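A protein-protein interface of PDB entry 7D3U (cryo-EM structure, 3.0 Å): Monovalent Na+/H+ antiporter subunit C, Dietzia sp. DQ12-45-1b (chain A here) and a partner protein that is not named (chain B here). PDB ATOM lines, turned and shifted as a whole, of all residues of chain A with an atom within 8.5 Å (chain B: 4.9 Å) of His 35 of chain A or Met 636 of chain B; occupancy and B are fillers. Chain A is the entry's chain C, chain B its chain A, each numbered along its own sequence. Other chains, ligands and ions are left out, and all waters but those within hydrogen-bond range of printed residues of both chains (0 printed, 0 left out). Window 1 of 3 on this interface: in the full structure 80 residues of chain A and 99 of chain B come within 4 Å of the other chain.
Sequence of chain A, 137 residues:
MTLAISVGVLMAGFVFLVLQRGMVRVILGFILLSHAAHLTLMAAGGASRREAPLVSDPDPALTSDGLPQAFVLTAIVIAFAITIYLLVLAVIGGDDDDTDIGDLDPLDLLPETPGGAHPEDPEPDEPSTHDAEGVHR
Of the 11 printed residues of chain B, 6 touch a printed residue of chain A.
Met 11 of chain A touches none of the printed residues of chain B.
Printed residues of chain B within 4 Å of Leu 32 of chain A: Val 632 (3.8 Å).
Of the printed residues of chain B, His 38 of chain A touches Phe 640.
Of the printed residues of chain A, Leu 609 of chain B touches Ser 6 (3.7 Å) and Leu 10 (3.8 Å).
No residue of chain A comes within 4 Å of Ala 635 of chain B.
Met 636 of chain B touches just these residues of chain A: Leu 10 (3.7 Å), His 35 (3.2 Å) and Leu 39 (3.0 Å).
Ala 637 of chain B touches none of the printed residues of chain A.
Of the printed residues of chain A, Trp 639 of chain B touches Leu 3 (3.5 Å) and Ser 6 (3.5 Å).
Printed residues of chain A within 4 Å of Gln 652 of chain B: His 35 (3.5 Å) and Ile 76 (3.6 Å).
The nearest residue of chain B that does not touch His 35 of chain A is Gly 633 of chain B (4.2 Å).
The nearest residue of chain A that does not touch Met 636 of chain B is His 38 of chain A (4.4 Å).
The side-chain hydroxyl (OG) of Ser 34 of chain A is in hydrogen-bond range of a ring nitrogen (NE2) of His 38 of chain A, 2.7 Å away.
Leu 3 of chain A touches Trp 639 of chain B.
CB of Ser 6 of chain A touches CD2 of Leu 609 of chain B, at 3.7 Å.
NE1 of Trp 639 of chain B touches OG of Ser 6 of chain A, at 3.5 Å.
Leu 609 of chain B touches Leu 10 of chain A (CD2 to CD1, 3.8 Å).
Leu 10 of chain A touches Met 636 of chain B.
Met 636 of chain B touches His 35 of chain A (CE to O, 3.2 Å).
CD2 of Leu 39 of chain A touches CE1 of Phe 640 of chain B (3.9 Å).
Phe 640 of chain B touches Met 42 of chain A.
CG2 of Val 72 of chain A touches CZ of Phe 640 of chain B (3.8 Å).
Ile 76 of chain A touches Gln 652 of chain B (CD1 to NE2, 3.6 Å).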
ATOM      1  N   LEU A   3      16.586 -29.190  22.115  1.00  0.00           N
ATOM      2  CA  LEU A   3      17.923 -28.828  22.563  1.00  0.00           C
ATOM      3  C   LEU A   3      18.999 -29.367  21.634  1.00  0.00           C
ATOM      4  O   LEU A   3      20.164 -28.985  21.767  1.00  0.00           O
ATOM      5  CB  LEU A   3      18.149 -29.327  23.988  1.00  0.00           C
ATOM      6  CG  LEU A   3      18.923 -28.390  24.912  1.00  0.00           C
ATOM      7  CD1 LEU A   3      18.602 -26.946  24.600  1.00  0.00           C
ATOM      8  CD2 LEU A   3      18.580 -28.695  26.354  1.00  0.00           C
ATOM      9  N   SER A   6      18.453 -26.687  18.255  1.00  0.00           N
ATOM     10  CA  SER A   6      19.045 -25.378  18.509  1.00  0.00           C
ATOM     11  C   SER A   6      20.566 -25.448  18.514  1.00  0.00           C
ATOM     12  O   SER A   6      21.236 -24.555  17.984  1.00  0.00           O
ATOM     13  CB  SER A   6      18.524 -24.815  19.828  1.00  0.00           C
ATOM     14  OG  SER A   6      18.946 -25.612  20.916  1.00  0.00           O
ATOM     15  N   VAL A   7      21.132 -26.506  19.098  1.00  0.00           N
ATOM     16  CA  VAL A   7      22.585 -26.654  19.098  1.00  0.00           C
ATOM     17  C   VAL A   7      23.101 -26.837  17.679  1.00  0.00           C
ATOM     18  O   VAL A   7      24.128 -26.263  17.303  1.00  0.00           O
ATOM     19  CB  VAL A   7      23.011 -27.819  20.008  1.00  0.00           C
ATOM     20  CG1 VAL A   7      24.436 -28.224  19.703  1.00  0.00           C
ATOM     21  CG2 VAL A   7      22.888 -27.421  21.458  1.00  0.00           C
ATOM     22  N   LEU A  10      22.974 -23.430  15.924  1.00  0.00           N
ATOM     23  CA  LEU A  10      24.037 -22.546  16.393  1.00  0.00           C
ATOM     24  C   LEU A  10      25.398 -22.996  15.881  1.00  0.00           C
ATOM     25  O   LEU A  10      26.236 -22.164  15.517  1.00  0.00           O
ATOM     26  CB  LEU A  10      24.031 -22.481  17.918  1.00  0.00           C
ATOM     27  CG  LEU A  10      22.885 -21.687  18.537  1.00  0.00           C
ATOM     28  CD1 LEU A  10      22.922 -21.802  20.046  1.00  0.00           C
ATOM     29  CD2 LEU A  10      22.956 -20.236  18.112  1.00  0.00           C
ATOM     30  N   MET A  11      25.639 -24.307  15.835  1.00  0.00           N
ATOM     31  CA  MET A  11      26.913 -24.802  15.330  1.00  0.00           C
ATOM     32  C   MET A  11      27.057 -24.530  13.840  1.00  0.00           C
ATOM     33  O   MET A  11      28.149 -24.194  13.370  1.00  0.00           O
ATOM     34  CB  MET A  11      27.050 -26.294  15.620  1.00  0.00           C
ATOM     35  CG  MET A  11      27.407 -26.609  17.059  1.00  0.00           C
ATOM     36  SD  MET A  11      29.053 -26.037  17.500  1.00  0.00           S
ATOM     37  CE  MET A  11      30.019 -26.760  16.179  1.00  0.00           C
ATOM     38  N   PHE A  14      27.916 -20.902  13.522  1.00  0.00           N
ATOM     39  CA  PHE A  14      29.320 -20.688  13.855  1.00  0.00           C
ATOM     40  C   PHE A  14      30.225 -21.112  12.710  1.00  0.00           C
ATOM     41  O   PHE A  14      31.129 -20.369  12.312  1.00  0.00           O
ATOM     42  CB  PHE A  14      29.695 -21.450  15.123  1.00  0.00           C
ATOM     43  CG  PHE A  14      31.110 -21.959  15.117  1.00  0.00           C
ATOM     44  CD1 PHE A  14      32.178 -21.089  15.255  1.00  0.00           C
ATOM     45  CD2 PHE A  14      31.373 -23.307  14.962  1.00  0.00           C
ATOM     46  CE1 PHE A  14      33.473 -21.554  15.243  1.00  0.00           C
ATOM     47  CE2 PHE A  14      32.669 -23.775  14.948  1.00  0.00           C
ATOM     48  CZ  PHE A  14      33.719 -22.897  15.089  1.00  0.00           C
ATOM     49  N   LEU A  28      31.490 -13.094  15.790  1.00  0.00           N
ATOM     50  CA  LEU A  28      30.089 -13.491  15.894  1.00  0.00           C
ATOM     51  C   LEU A  28      29.944 -15.004  15.807  1.00  0.00           C
ATOM     52  O   LEU A  28      29.145 -15.607  16.537  1.00  0.00           O
ATOM     53  CB  LEU A  28      29.258 -12.817  14.805  1.00  0.00           C
ATOM     54  CG  LEU A  28      29.343 -11.297  14.690  1.00  0.00           C
ATOM     55  CD1 LEU A  28      28.326 -10.798  13.694  1.00  0.00           C
ATOM     56  CD2 LEU A  28      29.169 -10.623  16.036  1.00  0.00           C
ATOM     57  N   GLY A  29      30.708 -15.636  14.916  1.00  0.00           N
ATOM     58  CA  GLY A  29      30.696 -17.086  14.851  1.00  0.00           C
ATOM     59  C   GLY A  29      31.177 -17.721  16.139  1.00  0.00           C
ATOM     60  O   GLY A  29      30.636 -18.733  16.585  1.00  0.00           O
ATOM     61  N   PHE A  30      32.194 -17.128  16.761  1.00  0.00           N
ATOM     62  CA  PHE A  30      32.667 -17.660  18.035  1.00  0.00           C
ATOM     63  C   PHE A  30      31.646 -17.447  19.146  1.00  0.00           C
ATOM     64  O   PHE A  30      31.534 -18.282  20.050  1.00  0.00           O
ATOM     65  CB  PHE A  30      34.007 -17.035  18.406  1.00  0.00           C
ATOM     66  CG  PHE A  30      35.174 -17.679  17.725  1.00  0.00           C
ATOM     67  CD1 PHE A  30      35.454 -19.016  17.930  1.00  0.00           C
ATOM     68  CD2 PHE A  30      35.985 -16.955  16.874  1.00  0.00           C
ATOM     69  CE1 PHE A  30      36.521 -19.616  17.304  1.00  0.00           C
ATOM     70  CE2 PHE A  30      37.054 -17.552  16.248  1.00  0.00           C
ATOM     71  CZ  PHE A  30      37.321 -18.884  16.462  1.00  0.00           C
ATOM     72  N   ILE A  31      30.884 -16.355  19.088  1.00  0.00           N
ATOM     73  CA  ILE A  31      29.797 -16.152  20.042  1.00  0.00           C
ATOM     74  C   ILE A  31      28.744 -17.239  19.876  1.00  0.00           C
ATOM     75  O   ILE A  31      28.258 -17.820  20.856  1.00  0.00           O
ATOM     76  CB  ILE A  31      29.188 -14.749  19.872  1.00  0.00           C
ATOM     77  CG1 ILE A  31      30.154 -13.683  20.380  1.00  0.00           C
ATOM     78  CG2 ILE A  31      27.867 -14.648  20.605  1.00  0.00           C
ATOM     79  CD1 ILE A  31      29.669 -12.278  20.151  1.00  0.00           C
ATOM     80  N   LEU A  32      28.379 -17.534  18.627  1.00  0.00           N
ATOM     81  CA  LEU A  32      27.404 -18.592  18.377  1.00  0.00           C
ATOM     82  C   LEU A  32      27.936 -19.949  18.823  1.00  0.00           C
ATOM     83  O   LEU A  32      27.182 -20.784  19.334  1.00  0.00           O
ATOM     84  CB  LEU A  32      27.030 -18.624  16.898  1.00  0.00           C
ATOM     85  CG  LEU A  32      26.190 -17.459  16.382  1.00  0.00           C
ATOM     86  CD1 LEU A  32      25.494 -17.847  15.093  1.00  0.00           C
ATOM     87  CD2 LEU A  32      25.180 -17.018  17.423  1.00  0.00           C
ATOM     88  N   LEU A  33      29.235 -20.184  18.646  1.00  0.00           N
ATOM     89  CA  LEU A  33      29.822 -21.452  19.067  1.00  0.00           C
ATOM     90  C   LEU A  33      29.817 -21.585  20.585  1.00  0.00           C
ATOM     91  O   LEU A  33      29.537 -22.664  21.121  1.00  0.00           O
ATOM     92  CB  LEU A  33      31.240 -21.570  18.521  1.00  0.00           C
ATOM     93  CG  LEU A  33      32.144 -22.640  19.122  1.00  0.00           C
ATOM     94  CD1 LEU A  33      31.740 -24.017  18.641  1.00  0.00           C
ATOM     95  CD2 LEU A  33      33.597 -22.360  18.794  1.00  0.00           C
ATOM     96  N   SER A  34      30.134 -20.499  21.292  1.00  0.00           N
ATOM     97  CA  SER A  34      30.035 -20.512  22.746  1.00  0.00           C
ATOM     98  C   SER A  34      28.602 -20.760  23.191  1.00  0.00           C
ATOM     99  O   SER A  34      28.360 -21.490  24.160  1.00  0.00           O
ATOM    100  CB  SER A  34      30.554 -19.195  23.319  1.00  0.00           C
ATOM    101  OG  SER A  34      29.942 -18.908  24.563  1.00  0.00           O
ATOM    102  N   HIS A  35      27.633 -20.162  22.492  1.00  0.00           N
ATOM    103  CA  HIS A  35      26.231 -20.422  22.803  1.00  0.00           C
ATOM    104  C   HIS A  35      25.890 -21.893  22.613  1.00  0.00           C
ATOM    105  O   HIS A  35      25.186 -22.489  23.436  1.00  0.00           O
ATOM    106  CB  HIS A  35      25.329 -19.551  21.933  1.00  0.00           C
ATOM    107  CG  HIS A  35      25.207 -18.139  22.410  1.00  0.00           C
ATOM    108  ND1 HIS A  35      25.378 -17.783  23.729  1.00  0.00           N
ATOM    109  CD2 HIS A  35      24.928 -16.995  21.744  1.00  0.00           C
ATOM    110  CE1 HIS A  35      25.212 -16.479  23.856  1.00  0.00           C
ATOM    111  NE2 HIS A  35      24.938 -15.977  22.666  1.00  0.00           N
ATOM    112  N   ALA A  36      26.381 -22.497  21.530  1.00  0.00           N
ATOM    113  CA  ALA A  36      26.120 -23.911  21.286  1.00  0.00           C
ATOM    114  C   ALA A  36      26.731 -24.780  22.375  1.00  0.00           C
ATOM    115  O   ALA A  36      26.117 -25.756  22.820  1.00  0.00           O
ATOM    116  CB  ALA A  36      26.657 -24.315  19.915  1.00  0.00           C
ATOM    117  N   ALA A  37      27.945 -24.443  22.815  1.00  0.00           N
ATOM    118  CA  ALA A  37      28.579 -25.208  23.884  1.00  0.00           C
ATOM    119  C   ALA A  37      27.803 -25.082  25.187  1.00  0.00           C
ATOM    120  O   ALA A  37      27.617 -26.068  25.908  1.00  0.00           O
ATOM    121  CB  ALA A  37      30.020 -24.750  24.080  1.00  0.00           C
ATOM    122  N   HIS A  38      27.336 -23.875  25.504  1.00  0.00           N
ATOM    123  CA  HIS A  38      26.535 -23.692  26.708  1.00  0.00           C
ATOM    124  C   HIS A  38      25.233 -24.474  26.624  1.00  0.00           C
ATOM    125  O   HIS A  38      24.782 -25.061  27.615  1.00  0.00           O
ATOM    126  CB  HIS A  38      26.257 -22.208  26.924  1.00  0.00           C
ATOM    127  CG  HIS A  38      27.494 -21.372  26.980  1.00  0.00           C
ATOM    128  ND1 HIS A  38      28.732 -21.898  27.280  1.00  0.00           N
ATOM    129  CD2 HIS A  38      27.688 -20.051  26.759  1.00  0.00           C
ATOM    130  CE1 HIS A  38      29.634 -20.934  27.250  1.00  0.00           C
ATOM    131  NE2 HIS A  38      29.027 -19.805  26.938  1.00  0.00           N
ATOM    132  N   LEU A  39      24.621 -24.507  25.442  1.00  0.00           N
ATOM    133  CA  LEU A  39      23.362 -25.225  25.289  1.00  0.00           C
ATOM    134  C   LEU A  39      23.561 -26.731  25.413  1.00  0.00           C
ATOM    135  O   LEU A  39      22.738 -27.419  26.025  1.00  0.00           O
ATOM    136  CB  LEU A  39      22.720 -24.868  23.952  1.00  0.00           C
ATOM    137  CG  LEU A  39      22.281 -23.415  23.791  1.00  0.00           C
ATOM    138  CD1 LEU A  39      21.800 -23.160  22.380  1.00  0.00           C
ATOM    139  CD2 LEU A  39      21.186 -23.100  24.784  1.00  0.00           C
ATOM    140  N   THR A  40      24.648 -27.269  24.850  1.00  0.00           N
ATOM    141  CA  THR A  40      24.876 -28.704  24.996  1.00  0.00           C
ATOM    142  C   THR A  40      25.343 -29.053  26.401  1.00  0.00           C
ATOM    143  O   THR A  40      25.205 -30.205  26.827  1.00  0.00           O
ATOM    144  CB  THR A  40      25.880 -29.222  23.967  1.00  0.00           C
ATOM    145  OG1 THR A  40      26.172 -30.594  24.251  1.00  0.00           O
ATOM    146  CG2 THR A  40      27.165 -28.456  24.039  1.00  0.00           C
ATOM    147  N   LEU A  41      25.904 -28.086  27.132  1.00  0.00           N
ATOM    148  CA  LEU A  41      26.175 -28.312  28.547  1.00  0.00           C
ATOM    149  C   LEU A  41      24.881 -28.371  29.345  1.00  0.00           C
ATOM    150  O   LEU A  41      24.724 -29.227  30.222  1.00  0.00           O
ATOM    151  CB  LEU A  41      27.087 -27.217  29.095  1.00  0.00           C
ATOM    152  CG  LEU A  41      28.544 -27.588  29.356  1.00  0.00           C
ATOM    153  CD1 LEU A  41      29.314 -26.366  29.803  1.00  0.00           C
ATOM    154  CD2 LEU A  41      28.629 -28.680  30.402  1.00  0.00           C
ATOM    155  N   MET A  42      23.942 -27.469  29.054  1.00  0.00           N
ATOM    156  CA  MET A  42      22.645 -27.518  29.721  1.00  0.00           C
ATOM    157  C   MET A  42      21.858 -28.761  29.326  1.00  0.00           C
ATOM    158  O   MET A  42      21.016 -29.229  30.099  1.00  0.00           O
ATOM    159  CB  MET A  42      21.837 -26.260  29.409  1.00  0.00           C
ATOM    160  CG  MET A  42      22.189 -25.070  30.277  1.00  0.00           C
ATOM    161  SD  MET A  42      22.162 -25.446  32.036  1.00  0.00           S
ATOM    162  CE  MET A  42      20.473 -25.997  32.240  1.00  0.00           C
ATOM    163  N   VAL A  72      28.095 -24.090  32.743  1.00  0.00           N
ATOM    164  CA  VAL A  72      27.783 -23.048  31.769  1.00  0.00           C
ATOM    165  C   VAL A  72      27.960 -21.668  32.390  1.00  0.00           C
ATOM    166  O   VAL A  72      28.378 -20.728  31.710  1.00  0.00           O
ATOM    167  CB  VAL A  72      26.368 -23.233  31.185  1.00  0.00           C
ATOM    168  CG1 VAL A  72      25.361 -23.478  32.266  1.00  0.00           C
ATOM    169  CG2 VAL A  72      25.957 -22.017  30.385  1.00  0.00           C
ATOM    170  N   ALA A  75      31.674 -21.117  31.964  1.00  0.00           N
ATOM    171  CA  ALA A  75      32.073 -21.020  30.566  1.00  0.00           C
ATOM    172  C   ALA A  75      31.562 -19.740  29.923  1.00  0.00           C
ATOM    173  O   ALA A  75      32.206 -19.213  29.012  1.00  0.00           O
ATOM    174  CB  ALA A  75      31.574 -22.238  29.794  1.00  0.00           C
ATOM    175  N   ILE A  76      30.425 -19.217  30.386  1.00  0.00           N
ATOM    176  CA  ILE A  76      29.909 -17.961  29.853  1.00  0.00           C
ATOM    177  C   ILE A  76      30.885 -16.831  30.138  1.00  0.00           C
ATOM    178  O   ILE A  76      31.222 -16.040  29.251  1.00  0.00           O
ATOM    179  CB  ILE A  76      28.517 -17.660  30.434  1.00  0.00           C
ATOM    180  CG1 ILE A  76      27.442 -18.439  29.682  1.00  0.00           C
ATOM    181  CG2 ILE A  76      28.218 -16.181  30.362  1.00  0.00           C
ATOM    182  CD1 ILE A  76      26.050 -18.208  30.206  1.00  0.00           C
ATOM    183  N   ALA A  79      34.158 -17.341  28.015  1.00  0.00           N
ATOM    184  CA  ALA A  79      33.955 -16.960  26.624  1.00  0.00           C
ATOM    185  C   ALA A  79      33.713 -15.467  26.482  1.00  0.00           C
ATOM    186  O   ALA A  79      34.078 -14.880  25.463  1.00  0.00           O
ATOM    187  CB  ALA A  79      32.788 -17.745  26.029  1.00  0.00           C
ATOM    188  N   LEU B 609      15.365 -18.670  18.138  1.00  0.00           N
ATOM    189  CA  LEU B 609      16.813 -18.811  18.033  1.00  0.00           C
ATOM    190  C   LEU B 609      17.238 -19.082  16.597  1.00  0.00           C
ATOM    191  O   LEU B 609      18.241 -18.533  16.128  1.00  0.00           O
ATOM    192  CB  LEU B 609      17.299 -19.927  18.954  1.00  0.00           C
ATOM    193  CG  LEU B 609      18.811 -20.017  19.137  1.00  0.00           C
ATOM    194  CD1 LEU B 609      19.351 -18.714  19.686  1.00  0.00           C
ATOM    195  CD2 LEU B 609      19.159 -21.170  20.055  1.00  0.00           C
ATOM    196  N   VAL B 632      19.997 -13.113  19.740  1.00  0.00           N
ATOM    197  CA  VAL B 632      20.395 -14.483  20.041  1.00  0.00           C
ATOM    198  C   VAL B 632      20.758 -14.616  21.513  1.00  0.00           C
ATOM    199  O   VAL B 632      20.477 -15.640  22.143  1.00  0.00           O
ATOM    200  CB  VAL B 632      21.548 -14.919  19.119  1.00  0.00           C
ATOM    201  CG1 VAL B 632      22.215 -16.174  19.645  1.00  0.00           C
ATOM    202  CG2 VAL B 632      21.026 -15.155  17.717  1.00  0.00           C
ATOM    203  N   GLY B 633      21.367 -13.582  22.093  1.00  0.00           N
ATOM    204  CA  GLY B 633      21.624 -13.602  23.524  1.00  0.00           C
ATOM    205  C   GLY B 633      20.348 -13.652  24.340  1.00  0.00           C
ATOM    206  O   GLY B 633      20.249 -14.402  25.314  1.00  0.00           O
ATOM    207  N   PHE B 634      19.345 -12.867  23.944  1.00  0.00           N
ATOM    208  CA  PHE B 634      18.064 -12.906  24.642  1.00  0.00           C
ATOM    209  C   PHE B 634      17.383 -14.259  24.477  1.00  0.00           C
ATOM    210  O   PHE B 634      16.787 -14.781  25.426  1.00  0.00           O
ATOM    211  CB  PHE B 634      17.155 -11.789  24.135  1.00  0.00           C
ATOM    212  CG  PHE B 634      17.122 -10.590  25.026  1.00  0.00           C
ATOM    213  CD1 PHE B 634      18.076  -9.598  24.907  1.00  0.00           C
ATOM    214  CD2 PHE B 634      16.139 -10.454  25.986  1.00  0.00           C
ATOM    215  CE1 PHE B 634      18.048  -8.493  25.724  1.00  0.00           C
ATOM    216  CE2 PHE B 634      16.106  -9.350  26.807  1.00  0.00           C
ATOM    217  CZ  PHE B 634      17.061  -8.369  26.677  1.00  0.00           C
ATOM    218  N   ALA B 635      17.460 -14.841  23.279  1.00  0.00           N
ATOM    219  CA  ALA B 635      16.860 -16.149  23.055  1.00  0.00           C
ATOM    220  C   ALA B 635      17.577 -17.232  23.843  1.00  0.00           C
ATOM    221  O   ALA B 635      16.938 -18.166  24.332  1.00  0.00           O
ATOM    222  CB  ALA B 635      16.865 -16.485  21.565  1.00  0.00           C
ATOM    223  N   MET B 636      18.895 -17.115  24.007  1.00  0.00           N
ATOM    224  CA  MET B 636      19.622 -18.080  24.821  1.00  0.00           C
ATOM    225  C   MET B 636      19.322 -17.897  26.301  1.00  0.00           C
ATOM    226  O   MET B 636      19.307 -18.874  27.054  1.00  0.00           O
ATOM    227  CB  MET B 636      21.121 -17.960  24.564  1.00  0.00           C
ATOM    228  CG  MET B 636      21.551 -18.505  23.221  1.00  0.00           C
ATOM    229  SD  MET B 636      21.720 -20.292  23.261  1.00  0.00           S
ATOM    230  CE  MET B 636      22.933 -20.461  24.561  1.00  0.00           C
ATOM    231  N   ALA B 637      19.077 -16.662  26.737  1.00  0.00           N
ATOM    232  CA  ALA B 637      18.637 -16.452  28.111  1.00  0.00           C
ATOM    233  C   ALA B 637      17.264 -17.068  28.344  1.00  0.00           C
ATOM    234  O   ALA B 637      17.029 -17.713  29.373  1.00  0.00           O
ATOM    235  CB  ALA B 637      18.618 -14.963  28.436  1.00  0.00           C
ATOM    236  N   LEU B 638      16.343 -16.879  27.397  1.00  0.00           N
ATOM    237  CA  LEU B 638      15.044 -17.538  27.480  1.00  0.00           C
ATOM    238  C   LEU B 638      15.191 -19.055  27.457  1.00  0.00           C
ATOM    239  O   LEU B 638      14.432 -19.764  28.126  1.00  0.00           O
ATOM    240  CB  LEU B 638      14.151 -17.069  26.333  1.00  0.00           C
ATOM    241  CG  LEU B 638      12.787 -17.736  26.171  1.00  0.00           C
ATOM    242  CD1 LEU B 638      11.972 -17.597  27.438  1.00  0.00           C
ATOM    243  CD2 LEU B 638      12.048 -17.135  24.992  1.00  0.00           C
ATOM    244  N   TRP B 639      16.164 -19.563  26.702  1.00  0.00           N
ATOM    245  CA  TRP B 639      16.446 -20.993  26.687  1.00  0.00           C
ATOM    246  C   TRP B 639      16.884 -21.476  28.062  1.00  0.00           C
ATOM    247  O   TRP B 639      16.337 -22.446  28.598  1.00  0.00           O
ATOM    248  CB  TRP B 639      17.529 -21.290  25.650  1.00  0.00           C
ATOM    249  CG  TRP B 639      17.143 -22.261  24.582  1.00  0.00           C
ATOM    250  CD1 TRP B 639      17.391 -22.140  23.249  1.00  0.00           C
ATOM    251  CD2 TRP B 639      16.476 -23.517  24.752  1.00  0.00           C
ATOM    252  NE1 TRP B 639      16.907 -23.229  22.574  1.00  0.00           N
ATOM    253  CE2 TRP B 639      16.341 -24.090  23.475  1.00  0.00           C
ATOM    254  CE3 TRP B 639      15.973 -24.207  25.857  1.00  0.00           C
ATOM    255  CZ2 TRP B 639      15.725 -25.317  23.273  1.00  0.00           C
ATOM    256  CZ3 TRP B 639      15.364 -25.423  25.654  1.00  0.00           C
ATOM    257  CH2 TRP B 639      15.247 -25.967  24.373  1.00  0.00           C
ATOM    258  N   PHE B 640      17.885 -20.812  28.643  1.00  0.00           N
ATOM    259  CA  PHE B 640      18.380 -21.202  29.958  1.00  0.00           C
ATOM    260  C   PHE B 640      17.300 -21.089  31.019  1.00  0.00           C
ATOM    261  O   PHE B 640      17.290 -21.868  31.978  1.00  0.00           O
ATOM    262  CB  PHE B 640      19.581 -20.341  30.346  1.00  0.00           C
ATOM    263  CG  PHE B 640      20.809 -20.614  29.537  1.00  0.00           C
ATOM    264  CD1 PHE B 640      21.118 -21.897  29.137  1.00  0.00           C
ATOM    265  CD2 PHE B 640      21.657 -19.586  29.181  1.00  0.00           C
ATOM    266  CE1 PHE B 640      22.248 -22.147  28.393  1.00  0.00           C
ATOM    267  CE2 PHE B 640      22.789 -19.832  28.440  1.00  0.00           C
ATOM    268  CZ  PHE B 640      23.083 -21.114  28.046  1.00  0.00           C
ATOM    269  N   GLN B 652      23.445 -14.815  31.454  1.00  0.00           N
ATOM    270  CA  GLN B 652      23.406 -14.755  29.998  1.00  0.00           C
ATOM    271  C   GLN B 652      22.851 -13.423  29.517  1.00  0.00           C
ATOM    272  O   GLN B 652      23.395 -12.823  28.585  1.00  0.00           O
ATOM    273  CB  GLN B 652      22.577 -15.911  29.449  1.00  0.00           C
ATOM    274  CG  GLN B 652      22.393 -15.872  27.948  1.00  0.00           C
ATOM    275  CD  GLN B 652      23.699 -15.677  27.213  1.00  0.00           C
ATOM    276  OE1 GLN B 652      23.892 -14.679  26.523  1.00  0.00           O
ATOM    277  NE2 GLN B 652      24.606 -16.634  27.356  1.00  0.00           N
